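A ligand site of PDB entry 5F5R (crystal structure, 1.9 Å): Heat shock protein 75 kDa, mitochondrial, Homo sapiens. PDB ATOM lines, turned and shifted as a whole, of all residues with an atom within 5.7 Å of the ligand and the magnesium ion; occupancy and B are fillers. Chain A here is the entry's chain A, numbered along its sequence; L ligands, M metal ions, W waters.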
ATOM      1  N   GLU A  59      24.677  26.784  -1.656  1.00  0.00           N
ATOM      2  CA  GLU A  59      25.395  25.606  -1.173  1.00  0.00           C
ATOM      3  C   GLU A  59      24.608  24.334  -1.448  1.00  0.00           C
ATOM      4  O   GLU A  59      25.128  23.378  -2.032  1.00  0.00           O
ATOM      5  CB  GLU A  59      25.714  25.724   0.320  1.00  0.00           C
ATOM      6  CG  GLU A  59      26.762  26.769   0.649  1.00  0.00           C
ATOM      7  CD  GLU A  59      28.182  26.265   0.482  1.00  0.00           C
ATOM      8  OE1 GLU A  59      28.386  25.262  -0.242  1.00  0.00           O
ATOM      9  OE2 GLU A  59      29.116  26.958   0.924  1.00  0.00           O
ATOM     10  N   LEU A  60      23.311  24.380  -1.150  1.00  0.00           N
ATOM     11  CA  LEU A  60      22.456  23.209  -1.322  1.00  0.00           C
ATOM     12  C   LEU A  60      22.148  22.942  -2.794  1.00  0.00           C
ATOM     13  O   LEU A  60      22.081  21.787  -3.224  1.00  0.00           O
ATOM     14  CB  LEU A  60      21.155  23.355  -0.521  1.00  0.00           C
ATOM     15  CG  LEU A  60      21.318  23.522   0.997  1.00  0.00           C
ATOM     16  CD1 LEU A  60      19.984  23.321   1.707  1.00  0.00           C
ATOM     17  CD2 LEU A  60      22.377  22.574   1.552  1.00  0.00           C
ATOM     18  N   SER A  62      24.156  23.716  -5.275  1.00  0.00           N
ATOM     19  CA  SER A  62      25.407  23.182  -5.818  1.00  0.00           C
ATOM     20  C   SER A  62      25.555  21.698  -5.511  1.00  0.00           C
ATOM     21  O   SER A  62      25.951  20.916  -6.372  1.00  0.00           O
ATOM     22  CB  SER A  62      26.604  23.958  -5.265  1.00  0.00           C
ATOM     23  OG  SER A  62      26.654  25.262  -5.829  1.00  0.00           O
ATOM     24  N   ASN A  63      25.140  21.287  -4.318  1.00  0.00           N
ATOM     25  CA  ASN A  63      25.159  19.869  -3.960  1.00  0.00           C
ATOM     26  C   ASN A  63      24.127  19.043  -4.725  1.00  0.00           C
ATOM     27  O   ASN A  63      24.395  17.904  -5.124  1.00  0.00           O
ATOM     28  CB  ASN A  63      24.965  19.697  -2.450  1.00  0.00           C
ATOM     29  CG  ASN A  63      26.171  20.144  -1.652  1.00  0.00           C
ATOM     30  OD1 ASN A  63      27.275  20.273  -2.196  1.00  0.00           O
ATOM     31  ND2 ASN A  63      25.966  20.419  -0.366  1.00  0.00           N
ATOM     32  N   ALA A  64      22.955  19.624  -4.942  1.00  0.00           N
ATOM     33  CA  ALA A  64      21.935  18.981  -5.778  1.00  0.00           C
ATOM     34  C   ALA A  64      22.481  18.782  -7.184  1.00  0.00           C
ATOM     35  O   ALA A  64      22.273  17.740  -7.805  1.00  0.00           O
ATOM     36  CB  ALA A  64      20.667  19.818  -5.803  1.00  0.00           C
ATOM     37  N   ASP A  66      25.672  18.637  -8.133  1.00  0.00           N
ATOM     38  CA  ASP A  66      26.700  17.597  -8.071  1.00  0.00           C
ATOM     39  C   ASP A  66      26.043  16.216  -8.122  1.00  0.00           C
ATOM     40  O   ASP A  66      26.515  15.317  -8.815  1.00  0.00           O
ATOM     41  CB  ASP A  66      27.542  17.728  -6.791  1.00  0.00           C
ATOM     42  CG  ASP A  66      28.489  18.913  -6.814  1.00  0.00           C
ATOM     43  OD1 ASP A  66      28.804  19.410  -7.916  1.00  0.00           O
ATOM     44  OD2 ASP A  66      29.005  19.279  -5.742  1.00  0.00           O
ATOM     45  N   ALA A  67      24.996  16.026  -7.330  1.00  0.00           N
ATOM     46  CA  ALA A  67      24.346  14.728  -7.230  1.00  0.00           C
ATOM     47  C   ALA A  67      23.754  14.317  -8.580  1.00  0.00           C
ATOM     48  O   ALA A  67      23.721  13.128  -8.908  1.00  0.00           O
ATOM     49  CB  ALA A  67      23.255  14.760  -6.157  1.00  0.00           C
ATOM     50  N   ASP A 102      16.522  17.030  -4.914  1.00  0.00           N
ATOM     51  CA  ASP A 102      17.071  16.669  -6.213  1.00  0.00           C
ATOM     52  C   ASP A 102      16.750  15.218  -6.547  1.00  0.00           C
ATOM     53  O   ASP A 102      16.519  14.410  -5.651  1.00  0.00           O
ATOM     54  CB  ASP A 102      18.589  16.900  -6.240  1.00  0.00           C
ATOM     55  CG  ASP A 102      19.353  15.934  -5.349  1.00  0.00           C
ATOM     56  OD1 ASP A 102      19.893  16.387  -4.318  1.00  0.00           O
ATOM     57  OD2 ASP A 102      19.528  14.763  -5.755  1.00  0.00           O
ATOM     58  N   ILE A 105      21.898  11.253  -7.410  1.00  0.00           N
ATOM     59  CA  ILE A 105      22.511   9.961  -7.093  1.00  0.00           C
ATOM     60  C   ILE A 105      22.094   9.431  -5.725  1.00  0.00           C
ATOM     61  O   ILE A 105      22.129   8.229  -5.476  1.00  0.00           O
ATOM     62  CB  ILE A 105      24.055  10.044  -7.179  1.00  0.00           C
ATOM     63  CG1 ILE A 105      24.688   8.654  -7.082  1.00  0.00           C
ATOM     64  CG2 ILE A 105      24.597  10.955  -6.084  1.00  0.00           C
ATOM     65  CD1 ILE A 105      24.807   7.961  -8.417  1.00  0.00           C
ATOM     66  N   GLY A 106      21.769  10.348  -4.817  1.00  0.00           N
ATOM     67  CA  GLY A 106      21.375   9.973  -3.465  1.00  0.00           C
ATOM     68  C   GLY A 106      22.540   9.487  -2.610  1.00  0.00           C
ATOM     69  O   GLY A 106      23.682   9.500  -3.050  1.00  0.00           O
ATOM     70  N   MET A 107      22.220   8.968  -1.428  1.00  0.00           N
ATOM     71  CA  MET A 107      23.240   8.519  -0.476  1.00  0.00           C
ATOM     72  C   MET A 107      22.839   7.196   0.163  1.00  0.00           C
ATOM     73  O   MET A 107      21.681   7.016   0.536  1.00  0.00           O
ATOM     74  CB  MET A 107      23.466   9.584   0.607  1.00  0.00           C
ATOM     75  CG  MET A 107      24.264  10.792   0.143  1.00  0.00           C
ATOM     76  SD  MET A 107      24.499  12.039   1.413  1.00  0.00           S
ATOM     77  CE  MET A 107      22.944  12.920   1.315  1.00  0.00           C
ATOM     78  N   ASN A 115      29.311  11.341   4.817  1.00  0.00           N
ATOM     79  CA  ASN A 115      29.284  12.571   4.026  1.00  0.00           C
ATOM     80  C   ASN A 115      28.711  13.766   4.770  1.00  0.00           C
ATOM     81  O   ASN A 115      29.125  14.904   4.564  1.00  0.00           O
ATOM     82  CB  ASN A 115      28.510  12.354   2.723  1.00  0.00           C
ATOM     83  CG  ASN A 115      29.241  11.452   1.756  1.00  0.00           C
ATOM     84  OD1 ASN A 115      30.380  11.081   1.999  1.00  0.00           O
ATOM     85  ND2 ASN A 115      28.493  10.903   0.797  1.00  0.00           N
ATOM     86  N   LEU A 116      27.627  13.536   5.508  1.00  0.00           N
ATOM     87  CA  LEU A 116      26.971  14.613   6.255  1.00  0.00           C
ATOM     88  C   LEU A 116      27.496  14.758   7.675  1.00  0.00           C
ATOM     89  O   LEU A 116      27.003  15.588   8.440  1.00  0.00           O
ATOM     90  CB  LEU A 116      25.463  14.403   6.271  1.00  0.00           C
ATOM     91  CG  LEU A 116      24.764  14.352   4.915  1.00  0.00           C
ATOM     92  CD1 LEU A 116      23.261  14.302   5.112  1.00  0.00           C
ATOM     93  CD2 LEU A 116      25.164  15.548   4.057  1.00  0.00           C
ATOM     94  N   ARG A 121      35.302  17.916   3.358  1.00  0.00           N
ATOM     95  CA  ARG A 121      35.285  19.003   2.384  1.00  0.00           C
ATOM     96  C   ARG A 121      36.547  19.834   2.481  1.00  0.00           C
ATOM     97  O   ARG A 121      36.880  20.352   3.547  1.00  0.00           O
ATOM     98  CB  ARG A 121      34.056  19.902   2.566  1.00  0.00           C
ATOM     99  CG  ARG A 121      34.168  21.247   1.849  1.00  0.00           C
ATOM    100  CD  ARG A 121      32.803  21.907   1.628  1.00  0.00           C
ATOM    101  NE  ARG A 121      32.723  23.203   2.283  1.00  0.00           N
ATOM    102  CZ  ARG A 121      33.360  24.292   1.892  1.00  0.00           C
ATOM    103  NH1 ARG A 121      32.946  24.943   0.810  1.00  0.00           N
ATOM    104  NH2 ARG A 121      34.049  24.970   2.800  1.00  0.00           N
ATOM    105  N   SER A 122      37.182  20.077   1.339  1.00  0.00           N
ATOM    106  CA  SER A 122      38.519  20.663   1.323  1.00  0.00           C
ATOM    107  C   SER A 122      38.521  22.134   1.740  1.00  0.00           C
ATOM    108  O   SER A 122      39.439  22.590   2.418  1.00  0.00           O
ATOM    109  CB  SER A 122      39.167  20.491  -0.059  1.00  0.00           C
ATOM    110  OG  SER A 122      39.243  19.117  -0.400  1.00  0.00           O
ATOM    111  N   GLY A 123      37.467  22.862   1.378  1.00  0.00           N
ATOM    112  CA  GLY A 123      37.396  24.284   1.698  1.00  0.00           C
ATOM    113  C   GLY A 123      37.083  24.514   3.163  1.00  0.00           C
ATOM    114  O   GLY A 123      37.449  25.549   3.726  1.00  0.00           O
ATOM    115  N   VAL A 147      31.277  26.961   3.923  1.00  0.00           N
ATOM    116  CA  VAL A 147      31.268  25.817   4.817  1.00  0.00           C
ATOM    117  C   VAL A 147      30.320  24.724   4.327  1.00  0.00           C
ATOM    118  O   VAL A 147      30.044  23.766   5.046  1.00  0.00           O
ATOM    119  CB  VAL A 147      30.916  26.233   6.267  1.00  0.00           C
ATOM    120  CG1 VAL A 147      31.948  27.209   6.798  1.00  0.00           C
ATOM    121  CG2 VAL A 147      29.517  26.842   6.315  1.00  0.00           C
ATOM    122  N   GLY A 148      30.016  24.760   3.030  1.00  0.00           N
ATOM    123  CA  GLY A 148      29.287  23.690   2.372  1.00  0.00           C
ATOM    124  C   GLY A 148      27.970  23.350   3.045  1.00  0.00           C
ATOM    125  O   GLY A 148      27.152  24.238   3.326  1.00  0.00           O
ATOM    126  N   PHE A 149      27.722  22.050   3.202  1.00  0.00           N
ATOM    127  CA  PHE A 149      26.431  21.560   3.691  1.00  0.00           C
ATOM    128  C   PHE A 149      26.084  22.180   5.046  1.00  0.00           C
ATOM    129  O   PHE A 149      24.931  22.523   5.300  1.00  0.00           O
ATOM    130  CB  PHE A 149      26.463  20.041   3.809  1.00  0.00           C
ATOM    131  CG  PHE A 149      25.291  19.460   4.548  1.00  0.00           C
ATOM    132  CD1 PHE A 149      24.033  19.417   3.971  1.00  0.00           C
ATOM    133  CD2 PHE A 149      25.453  18.957   5.833  1.00  0.00           C
ATOM    134  CE1 PHE A 149      22.953  18.892   4.653  1.00  0.00           C
ATOM    135  CE2 PHE A 149      24.359  18.483   6.543  1.00  0.00           C
ATOM    136  CZ  PHE A 149      23.112  18.422   5.941  1.00  0.00           C
ATOM    137  N   TYR A 150      27.103  22.424   5.864  1.00  0.00           N
ATOM    138  CA  TYR A 150      26.884  22.910   7.227  1.00  0.00           C
ATOM    139  C   TYR A 150      26.420  24.363   7.250  1.00  0.00           C
ATOM    140  O   TYR A 150      25.986  24.861   8.292  1.00  0.00           O
ATOM    141  CB  TYR A 150      28.145  22.743   8.062  1.00  0.00           C
ATOM    142  CG  TYR A 150      28.462  21.303   8.373  1.00  0.00           C
ATOM    143  CD1 TYR A 150      29.525  20.672   7.743  1.00  0.00           C
ATOM    144  CD2 TYR A 150      27.529  20.511   9.038  1.00  0.00           C
ATOM    145  CE1 TYR A 150      29.706  19.303   7.855  1.00  0.00           C
ATOM    146  CE2 TYR A 150      27.669  19.135   9.098  1.00  0.00           C
ATOM    147  CZ  TYR A 150      28.747  18.535   8.484  1.00  0.00           C
ATOM    148  OH  TYR A 150      28.977  17.190   8.662  1.00  0.00           O
ATOM    149  N   SER A 163      17.144  10.470   1.956  1.00  0.00           N
ATOM    150  CA  SER A 163      17.983  10.102   0.815  1.00  0.00           C
ATOM    151  C   SER A 163      17.894   8.627   0.470  1.00  0.00           C
ATOM    152  O   SER A 163      17.751   7.776   1.360  1.00  0.00           O
ATOM    153  CB  SER A 163      19.440  10.518   1.041  1.00  0.00           C
ATOM    154  OG  SER A 163      20.166  10.512  -0.176  1.00  0.00           O
ATOM    155  N   THR A 195      17.756  13.041  -3.069  1.00  0.00           N
ATOM    156  CA  THR A 195      17.881  13.600  -1.731  1.00  0.00           C
ATOM    157  C   THR A 195      16.926  14.785  -1.549  1.00  0.00           C
ATOM    158  O   THR A 195      16.901  15.702  -2.365  1.00  0.00           O
ATOM    159  CB  THR A 195      19.327  14.062  -1.445  1.00  0.00           C
ATOM    160  OG1 THR A 195      20.223  12.965  -1.668  1.00  0.00           O
ATOM    161  CG2 THR A 195      19.460  14.537  -0.011  1.00  0.00           C
ATOM    162  N   ILE A 197      16.092  17.750   1.320  1.00  0.00           N
ATOM    163  CA  ILE A 197      16.570  18.387   2.542  1.00  0.00           C
ATOM    164  C   ILE A 197      15.569  19.420   3.046  1.00  0.00           C
ATOM    165  O   ILE A 197      15.249  20.380   2.345  1.00  0.00           O
ATOM    166  CB  ILE A 197      17.930  19.067   2.341  1.00  0.00           C
ATOM    167  CG1 ILE A 197      18.976  18.049   1.877  1.00  0.00           C
ATOM    168  CG2 ILE A 197      18.384  19.750   3.619  1.00  0.00           C
ATOM    169  CD1 ILE A 197      20.295  18.677   1.449  1.00  0.00           C
HETATM  170  P1  LIG L   1      32.196  21.908  -2.212  1.00  0.00           P
HETATM  171  O1  LIG L   1      30.780  22.191  -1.742  1.00  0.00           O
HETATM  172  O2  LIG L   1      33.223  22.787  -1.545  1.00  0.00           O
HETATM  173  O3  LIG L   1      32.330  21.824  -3.712  1.00  0.00           O
HETATM  174  P2  LIG L   1      31.303  19.212  -1.168  1.00  0.00           P
HETATM  175  O4  LIG L   1      30.061  19.447  -1.989  1.00  0.00           O
HETATM  176  O5  LIG L   1      31.903  17.831  -1.146  1.00  0.00           O
HETATM  177  N1  LIG L   1      32.561  20.295  -1.667  1.00  0.00           N
HETATM  178  P3  LIG L   1      29.494  19.805   0.966  1.00  0.00           P
HETATM  179  O6  LIG L   1      29.665  20.108   2.434  1.00  0.00           O
HETATM  180  O7  LIG L   1      28.737  20.773   0.096  1.00  0.00           O
HETATM  181  O8  LIG L   1      30.974  19.584   0.373  1.00  0.00           O
HETATM  182  O9  LIG L   1      28.826  18.359   0.836  1.00  0.00           O
HETATM  183  C1  LIG L   1      29.477  17.301   1.537  1.00  0.00           C
HETATM  184  C2  LIG L   1      29.108  15.955   0.942  1.00  0.00           C
HETATM  185  O10 LIG L   1      27.770  15.603   1.305  1.00  0.00           O
HETATM  186  C3  LIG L   1      29.116  15.942  -0.580  1.00  0.00           C
HETATM  187  O11 LIG L   1      30.425  15.700  -1.092  1.00  0.00           O
HETATM  188  C4  LIG L   1      28.180  14.785  -0.882  1.00  0.00           C
HETATM  189  O12 LIG L   1      28.920  13.562  -0.758  1.00  0.00           O
HETATM  190  C5  LIG L   1      27.176  14.838   0.260  1.00  0.00           C
HETATM  191  N2  LIG L   1      25.940  15.530  -0.193  1.00  0.00           N
HETATM  192  C6  LIG L   1      25.517  16.746   0.179  1.00  0.00           C
HETATM  193  N3  LIG L   1      24.347  17.068  -0.443  1.00  0.00           N
HETATM  194  C7  LIG L   1      23.975  15.989  -1.165  1.00  0.00           C
HETATM  195  C8  LIG L   1      22.930  15.699  -2.169  1.00  0.00           C
HETATM  196  N4  LIG L   1      21.917  16.568  -2.403  1.00  0.00           N
HETATM  197  N5  LIG L   1      22.950  14.479  -2.758  1.00  0.00           N
HETATM  198  C9  LIG L   1      23.965  13.614  -2.572  1.00  0.00           C
HETATM  199  N6  LIG L   1      24.968  13.829  -1.708  1.00  0.00           N
HETATM  200  C10 LIG L   1      25.045  14.999  -1.023  1.00  0.00           C
HETATM  201 MG    MG M   1      29.009  21.212  -1.844  1.00  0.00          MG
HETATM  202  O   HOH W   1      35.772  22.288  -1.026  1.00  0.00           O
HETATM  203  O   HOH W   2      35.223  19.612  -1.869  1.00  0.00           O
HETATM  204  O   HOH W   3      21.026  13.173  -4.165  1.00  0.00           O
HETATM  205  O   HOH W   4      33.496  16.751   0.780  1.00  0.00           O
HETATM  206  O   HOH W   5      34.123  25.195  -2.509  1.00  0.00           O
HETATM  207  O   HOH W   6      26.277  16.364  -3.605  1.00  0.00           O
HETATM  208  O   HOH W   7      28.956  21.464  -3.972  1.00  0.00           O
HETATM  209  O   HOH W   8      30.925  19.286   4.579  1.00  0.00           O
HETATM  210  O   HOH W   9      27.077  11.844  -1.540  1.00  0.00           O
HETATM  211  O   HOH W  10      32.709  17.238  -3.635  1.00  0.00           O
HETATM  212  O   HOH W  11      27.840  23.002  -1.548  1.00  0.00           O
HETATM  213  O   HOH W  12      30.921  24.881  -1.108  1.00  0.00           O
HETATM  214  O   HOH W  13      34.651  22.341  -4.852  1.00  0.00           O
HETATM  215  O   HOH W  14      28.778  17.576  -3.607  1.00  0.00           O
HETATM  216  O   HOH W  15      23.248  19.520   0.371  1.00  0.00           O
HETATM  217  O   HOH W  16      30.879  23.461  -5.128  1.00  0.00           O
HETATM  218  O   HOH W  17      21.300  19.531  -1.771  1.00  0.00           O
HETATM  219  O   HOH W  18      18.885  18.248  -2.626  1.00  0.00           O
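The side-chain sulfur of Met 107 lies close to a nitrogen (N6) of the ligand. Asp 66 touches the ligand (OD2 to O4, 3.9 Å). Ala 67 touches the ligand. CD2 of Leu 116 touches O10 of the ligand (3.8 Å). Gly 148 touches the ligand (CA to O6, 3.6 Å). Within 4 Å of the ligand: Asn 63, Asp 66, Ala 67, Asp 102, Met 107, Asn 115, Leu 116, Arg 121, Gly 148, Phe 149 and Thr 195. Along chain A the residues within 4 Å of the ligand span positions 63 to 195.
Within 4 Å of the magnesium ion: Asn 63.
OD1 of Asp 102 is in hydrogen-bond range of N4 of the ligand. An oxygen (O6) of the ligand lies within hydrogen-bond range of the backbone NH of Phe 149 (2.9 Å). O12 of the ligand sits at hydrogen-bond distance from ND2 of Asn 115. The guanidinium group (NH1) of Arg 121 lies within salt-bridge range of an oxygen (O2) of the ligand (3.2 Å). The side-chain hydroxyl (OG1) of Thr 195 lies within hydrogen-bond range of a nitrogen (N5) of the ligand (3.3 Å).
Water W7 lies within hydrogen-bond range of the side-chain carboxylate of Asp 66 and an oxygen (O3) of the ligand. Water W11 lies within hydrogen-bond range of OE1 of Glu 59 (2.7 Å) and ND2 of Asn 63 (3.4 Å). Water W3 lies within hydrogen-bond range of OG1 of Thr 195 (2.6 Å), OD2 of Asp 102 (2.7 Å), N5 of the ligand (2.7 Å) and N of Gly 106 (3.0 Å). Water W4 lies within hydrogen-bond range of an oxygen (O5) of the ligand (2.7 Å) and the backbone NH (N) of Arg 121 (3.4 Å). Water W12 lies within hydrogen-bond range of the side-chain carboxylate of Glu 59 (2.7 Å), the guanidinium group of Arg 121 (2.8 Å) and an oxygen (O2) of the ligand (3.1 Å). Water W18 lies within hydrogen-bond range of OD1 of Asp 102 (2.7 Å), O of Thr 195 (3.2 Å) and N4 of the ligand (3.5 Å).
The magnesium ion is bound by OD1 of Asn 63 (2.0 Å), O7 of the ligand (2.0 Å), O1 of the ligand (2.0 Å), O4 of the ligand (2.1 Å), water W7 (2.1 Å) and water W11 (2.2 Å).
ND2 of Asn 63 sits close to O of Glu 59, 3.5 Å away. The backbone NH (N) of Asp 102 is in hydrogen-bond range of the backbone carbonyl oxygen (O) of Thr 195. The side-chain hydroxyl (OG1) of Thr 195 lies within hydrogen-bond range of the side-chain hydroxyl (OG) of Ser 163, at 2.9 Å. O of Ala 67 sits at hydrogen-bond distance from N of Ile 105, 3.0 Å away. The backbone NH (N) of Gly 148 sits at hydrogen-bond distance from the side-chain carboxylate (OE2) of Glu 59, at 3.2 Å. The backbone NH (N) of Met 107 lies within hydrogen-bond range of the side-chain hydroxyl (OG) of Ser 163 (2.9 Å). OH of Tyr 150 lies within hydrogen-bond range of O of Leu 116 (2.6 Å).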
